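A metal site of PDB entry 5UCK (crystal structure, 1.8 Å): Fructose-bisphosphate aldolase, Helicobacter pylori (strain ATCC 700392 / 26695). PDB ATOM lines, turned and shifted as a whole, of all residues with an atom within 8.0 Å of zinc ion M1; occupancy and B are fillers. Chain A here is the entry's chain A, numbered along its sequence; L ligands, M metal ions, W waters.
The backbone NH (N) of Gly 211 sits at hydrogen-bond distance from an oxygen (O5) of the ligand.
The side-chain carboxylate (OD1) of Asp 82 lies close to an oxygen (O6) of the ligand (3.1 Å).
An oxygen (O6) of the ligand lies close to the side-chain amide nitrogen (ND2) of Asn 253 (2.9 Å).
The backbone carbonyl oxygen (O) of His 210 lies within hydrogen-bond range of the side-chain hydroxyl (OG1) of Thr 178, 2.7 Å away.
NE2 of His 210 sits at hydrogen-bond distance from OE2 of Glu 132 (2.7 Å).
A ring nitrogen (ND1) of His 83 lies within hydrogen-bond range of the side-chain carboxylate of Asp 82 (2.8 Å).
The side-chain sulfur (SD) of Met 102 sits at hydrogen-bond distance from the backbone NH (N) of His 83 (3.4 Å).
Residues that only touch zinc ion M1: His 180 (3.5 Å).
Of the 19 residues printed, 4 come within 4 Å of zinc ion M1.
Zinc ion M1 is bound by water W1, NE2 of His 83, ND1 of His 210 and OE2 of Glu 134.
Water W1 lies within hydrogen-bond range of the side-chain carboxylate (OD2) of Asp 104 (2.5 Å) and the side-chain carboxylate (OE1) of Glu 134 (2.8 Å).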
ATOM      1  N   ASP A  82      26.181  25.373   9.195  1.00  0.00           N
ATOM      2  CA  ASP A  82      26.609  25.302   7.812  1.00  0.00           C
ATOM      3  C   ASP A  82      26.479  23.868   7.282  1.00  0.00           C
ATOM      4  O   ASP A  82      27.072  22.945   7.849  1.00  0.00           O
ATOM      5  CB  ASP A  82      28.052  25.794   7.736  1.00  0.00           C
ATOM      6  CG  ASP A  82      28.593  25.845   6.345  1.00  0.00           C
ATOM      7  OD1 ASP A  82      27.805  25.928   5.381  1.00  0.00           O
ATOM      8  OD2 ASP A  82      29.836  25.808   6.242  1.00  0.00           O
ATOM      9  N   HIS A  83      25.699  23.696   6.218  1.00  0.00           N
ATOM     10  CA  HIS A  83      25.513  22.411   5.549  1.00  0.00           C
ATOM     11  C   HIS A  83      25.096  21.311   6.525  1.00  0.00           C
ATOM     12  O   HIS A  83      25.745  20.277   6.666  1.00  0.00           O
ATOM     13  CB  HIS A  83      26.769  21.993   4.781  1.00  0.00           C
ATOM     14  CG  HIS A  83      26.947  22.715   3.479  1.00  0.00           C
ATOM     15  ND1 HIS A  83      27.454  23.986   3.392  1.00  0.00           N
ATOM     16  CD2 HIS A  83      26.673  22.325   2.201  1.00  0.00           C
ATOM     17  CE1 HIS A  83      27.491  24.359   2.121  1.00  0.00           C
ATOM     18  NE2 HIS A  83      27.023  23.370   1.385  1.00  0.00           N
ATOM     19  N   MET A 102      21.123  25.616   8.086  1.00  0.00           N
ATOM     20  CA  MET A 102      21.043  25.222   6.685  1.00  0.00           C
ATOM     21  C   MET A 102      20.768  23.733   6.599  1.00  0.00           C
ATOM     22  O   MET A 102      21.434  22.929   7.264  1.00  0.00           O
ATOM     23  CB  MET A 102      22.330  25.565   5.942  1.00  0.00           C
ATOM     24  CG  MET A 102      22.250  25.275   4.457  1.00  0.00           C
ATOM     25  SD  MET A 102      23.834  24.913   3.681  1.00  0.00           S
ATOM     26  CE  MET A 102      23.216  24.398   2.081  1.00  0.00           C
ATOM     27  N   ASP A 104      20.980  21.060   3.713  1.00  0.00           N
ATOM     28  CA  ASP A 104      21.444  20.832   2.344  1.00  0.00           C
ATOM     29  C   ASP A 104      20.862  19.520   1.864  1.00  0.00           C
ATOM     30  O   ASP A 104      21.330  18.437   2.238  1.00  0.00           O
ATOM     31  CB  ASP A 104      22.969  20.812   2.282  1.00  0.00           C
ATOM     32  CG  ASP A 104      23.477  20.623   0.874  1.00  0.00           C
ATOM     33  OD1 ASP A 104      22.657  20.580  -0.080  1.00  0.00           O
ATOM     34  OD2 ASP A 104      24.710  20.520   0.706  1.00  0.00           O
ATOM     35  N   SER A 106      20.124  19.411  -1.687  1.00  0.00           N
ATOM     36  CA  SER A 106      20.116  19.715  -3.120  1.00  0.00           C
ATOM     37  C   SER A 106      20.487  18.511  -3.978  1.00  0.00           C
ATOM     38  O   SER A 106      20.255  18.538  -5.188  1.00  0.00           O
ATOM     39  CB  SER A 106      21.071  20.881  -3.401  1.00  0.00           C
ATOM     40  OG  SER A 106      22.401  20.543  -3.078  1.00  0.00           O
ATOM     41  N   GLU A 132      18.203  28.231   5.833  1.00  0.00           N
ATOM     42  CA  GLU A 132      18.782  28.251   4.492  1.00  0.00           C
ATOM     43  C   GLU A 132      18.597  26.877   3.856  1.00  0.00           C
ATOM     44  O   GLU A 132      18.662  25.851   4.539  1.00  0.00           O
ATOM     45  CB  GLU A 132      20.273  28.594   4.544  1.00  0.00           C
ATOM     46  CG  GLU A 132      20.997  28.557   3.201  1.00  0.00           C
ATOM     47  CD  GLU A 132      22.485  28.777   3.338  1.00  0.00           C
ATOM     48  OE1 GLU A 132      22.905  29.619   4.166  1.00  0.00           O
ATOM     49  OE2 GLU A 132      23.245  28.110   2.607  1.00  0.00           O
ATOM     50  N   GLU A 134      19.272  24.750  -0.298  1.00  0.00           N
ATOM     51  CA  GLU A 134      20.085  24.784  -1.494  1.00  0.00           C
ATOM     52  C   GLU A 134      19.349  24.127  -2.646  1.00  0.00           C
ATOM     53  O   GLU A 134      18.692  23.103  -2.480  1.00  0.00           O
ATOM     54  CB  GLU A 134      21.427  24.066  -1.286  1.00  0.00           C
ATOM     55  CG  GLU A 134      22.353  24.163  -2.482  1.00  0.00           C
ATOM     56  CD  GLU A 134      23.783  23.819  -2.153  1.00  0.00           C
ATOM     57  OE1 GLU A 134      24.017  23.122  -1.138  1.00  0.00           O
ATOM     58  OE2 GLU A 134      24.684  24.247  -2.904  1.00  0.00           O
ATOM     59  N   LEU A 135      19.478  24.727  -3.829  1.00  0.00           N
ATOM     60  CA  LEU A 135      18.844  24.211  -5.034  1.00  0.00           C
ATOM     61  C   LEU A 135      19.847  24.279  -6.174  1.00  0.00           C
ATOM     62  O   LEU A 135      20.457  25.326  -6.401  1.00  0.00           O
ATOM     63  CB  LEU A 135      17.575  24.995  -5.371  1.00  0.00           C
ATOM     64  CG  LEU A 135      16.498  24.323  -6.227  1.00  0.00           C
ATOM     65  CD1 LEU A 135      15.978  23.057  -5.573  1.00  0.00           C
ATOM     66  CD2 LEU A 135      15.358  25.307  -6.477  1.00  0.00           C
ATOM     67  N   GLY A 136      20.005  23.176  -6.894  1.00  0.00           N
ATOM     68  CA  GLY A 136      21.021  23.060  -7.908  1.00  0.00           C
ATOM     69  C   GLY A 136      22.233  22.269  -7.426  1.00  0.00           C
ATOM     70  O   GLY A 136      22.438  22.052  -6.228  1.00  0.00           O
ATOM     71  N   ARG A 137      23.047  21.837  -8.381  1.00  0.00           N
ATOM     72  CA  ARG A 137      24.205  21.016  -8.087  1.00  0.00           C
ATOM     73  C   ARG A 137      25.425  21.478  -8.875  1.00  0.00           C
ATOM     74  O   ARG A 137      25.297  22.071  -9.943  1.00  0.00           O
ATOM     75  CB  ARG A 137      23.905  19.541  -8.383  1.00  0.00           C
ATOM     76  CG  ARG A 137      22.565  19.075  -7.857  1.00  0.00           C
ATOM     77  CD  ARG A 137      22.203  17.692  -8.367  1.00  0.00           C
ATOM     78  NE  ARG A 137      20.800  17.384  -8.114  1.00  0.00           N
ATOM     79  CZ  ARG A 137      20.228  16.210  -8.405  1.00  0.00           C
ATOM     80  NH1 ARG A 137      20.950  15.242  -8.944  1.00  0.00           N
ATOM     81  NH2 ARG A 137      18.944  16.026  -8.139  1.00  0.00           N
ATOM     82  N   ALA A 173      20.323  29.196  -1.377  1.00  0.00           N
ATOM     83  CA  ALA A 173      21.621  29.107  -2.036  1.00  0.00           C
ATOM     84  C   ALA A 173      21.432  28.489  -3.416  1.00  0.00           C
ATOM     85  O   ALA A 173      21.334  27.262  -3.528  1.00  0.00           O
ATOM     86  CB  ALA A 173      22.593  28.267  -1.208  1.00  0.00           C
ATOM     87  N   ALA A 175      22.713  27.220  -7.103  1.00  0.00           N
ATOM     88  CA  ALA A 175      23.931  26.824  -7.809  1.00  0.00           C
ATOM     89  C   ALA A 175      24.101  27.685  -9.058  1.00  0.00           C
ATOM     90  O   ALA A 175      23.263  27.640  -9.963  1.00  0.00           O
ATOM     91  CB  ALA A 175      23.869  25.343  -8.180  1.00  0.00           C
ATOM     92  N   THR A 178      29.793  27.955  -8.383  1.00  0.00           N
ATOM     93  CA  THR A 178      30.833  27.824  -7.375  1.00  0.00           C
ATOM     94  C   THR A 178      30.925  26.391  -6.853  1.00  0.00           C
ATOM     95  O   THR A 178      30.133  25.513  -7.213  1.00  0.00           O
ATOM     96  CB  THR A 178      30.591  28.799  -6.215  1.00  0.00           C
ATOM     97  OG1 THR A 178      29.300  28.563  -5.648  1.00  0.00           O
ATOM     98  CG2 THR A 178      30.687  30.236  -6.689  1.00  0.00           C
ATOM     99  N   SER A 179      31.910  26.142  -5.992  1.00  0.00           N
ATOM    100  CA  SER A 179      32.106  24.844  -5.358  1.00  0.00           C
ATOM    101  C   SER A 179      32.996  25.032  -4.146  1.00  0.00           C
ATOM    102  O   SER A 179      33.764  25.991  -4.054  1.00  0.00           O
ATOM    103  CB  SER A 179      32.721  23.833  -6.335  1.00  0.00           C
ATOM    104  OG  SER A 179      34.054  24.186  -6.675  1.00  0.00           O
ATOM    105  N   HIS A 180      32.887  24.091  -3.204  1.00  0.00           N
ATOM    106  CA  HIS A 180      33.632  24.174  -1.961  1.00  0.00           C
ATOM    107  C   HIS A 180      35.139  24.088  -2.212  1.00  0.00           C
ATOM    108  O   HIS A 180      35.602  23.664  -3.272  1.00  0.00           O
ATOM    109  CB  HIS A 180      33.217  23.061  -1.003  1.00  0.00           C
ATOM    110  CG  HIS A 180      31.880  23.277  -0.366  1.00  0.00           C
ATOM    111  ND1 HIS A 180      31.271  22.325   0.431  1.00  0.00           N
ATOM    112  CD2 HIS A 180      31.044  24.343  -0.396  1.00  0.00           C
ATOM    113  CE1 HIS A 180      30.113  22.796   0.851  1.00  0.00           C
ATOM    114  NE2 HIS A 180      29.951  24.021   0.374  1.00  0.00           N
ATOM    115  N   LEU A 209      25.792  32.590  -1.458  1.00  0.00           N
ATOM    116  CA  LEU A 209      26.817  32.067  -2.351  1.00  0.00           C
ATOM    117  C   LEU A 209      27.763  31.156  -1.558  1.00  0.00           C
ATOM    118  O   LEU A 209      28.413  31.625  -0.610  1.00  0.00           O
ATOM    119  CB  LEU A 209      27.596  33.196  -3.021  1.00  0.00           C
ATOM    120  CG  LEU A 209      28.593  32.762  -4.091  1.00  0.00           C
ATOM    121  CD1 LEU A 209      27.863  32.249  -5.331  1.00  0.00           C
ATOM    122  CD2 LEU A 209      29.537  33.891  -4.461  1.00  0.00           C
ATOM    123  N   HIS A 210      27.802  29.873  -1.918  1.00  0.00           N
ATOM    124  CA  HIS A 210      28.737  28.935  -1.327  1.00  0.00           C
ATOM    125  C   HIS A 210      30.059  28.932  -2.105  1.00  0.00           C
ATOM    126  O   HIS A 210      30.127  29.372  -3.258  1.00  0.00           O
ATOM    127  CB  HIS A 210      28.187  27.501  -1.320  1.00  0.00           C
ATOM    128  CG  HIS A 210      26.962  27.330  -0.476  1.00  0.00           C
ATOM    129  ND1 HIS A 210      26.182  26.193  -0.538  1.00  0.00           N
ATOM    130  CD2 HIS A 210      26.376  28.137   0.439  1.00  0.00           C
ATOM    131  CE1 HIS A 210      25.172  26.303   0.314  1.00  0.00           C
ATOM    132  NE2 HIS A 210      25.270  27.474   0.921  1.00  0.00           N
ATOM    133  N   GLY A 211      31.103  28.429  -1.459  1.00  0.00           N
ATOM    134  CA  GLY A 211      32.405  28.322  -2.095  1.00  0.00           C
ATOM    135  C   GLY A 211      32.884  29.657  -2.621  1.00  0.00           C
ATOM    136  O   GLY A 211      33.329  29.759  -3.768  1.00  0.00           O
ATOM    137  N   ASN A 253      29.538  32.748   1.757  1.00  0.00           N
ATOM    138  CA  ASN A 253      30.185  31.751   2.606  1.00  0.00           C
ATOM    139  C   ASN A 253      31.693  31.770   2.383  1.00  0.00           C
ATOM    140  O   ASN A 253      32.171  31.632   1.250  1.00  0.00           O
ATOM    141  CB  ASN A 253      29.607  30.372   2.287  1.00  0.00           C
ATOM    142  CG  ASN A 253      28.265  30.124   2.960  1.00  0.00           C
ATOM    143  OD1 ASN A 253      27.515  31.054   3.264  1.00  0.00           O
ATOM    144  ND2 ASN A 253      27.938  28.857   3.195  1.00  0.00           N
HETATM  145  P1  LIG L   1      35.190  28.383   0.529  1.00  0.00           P
HETATM  146  O1  LIG L   1      35.913  27.061   0.451  1.00  0.00           O
HETATM  147  O2  LIG L   1      35.540  29.230   1.712  1.00  0.00           O
HETATM  148  O3  LIG L   1      35.128  29.124  -0.792  1.00  0.00           O
HETATM  149  O4  LIG L   1      33.662  27.944   0.798  1.00  0.00           O
HETATM  150  C1  LIG L   1      33.013  28.332   2.009  1.00  0.00           C
HETATM  151  C2  LIG L   1      31.713  27.595   2.115  1.00  0.00           C
HETATM  152  O5  LIG L   1      31.185  27.131   1.113  1.00  0.00           O
HETATM  153  C3  LIG L   1      31.040  27.428   3.449  1.00  0.00           C
HETATM  154  O6  LIG L   1      29.848  26.680   3.206  1.00  0.00           O
HETATM  155 ZN    ZN M   1      26.838  23.761  -1.165  1.00  0.00          ZN
HETATM  156 ZN    ZN M   2      28.986  25.511   1.363  1.00  0.00          ZN
HETATM  157  O   HOH W   1      26.239  21.499  -0.953  1.00  0.00           O
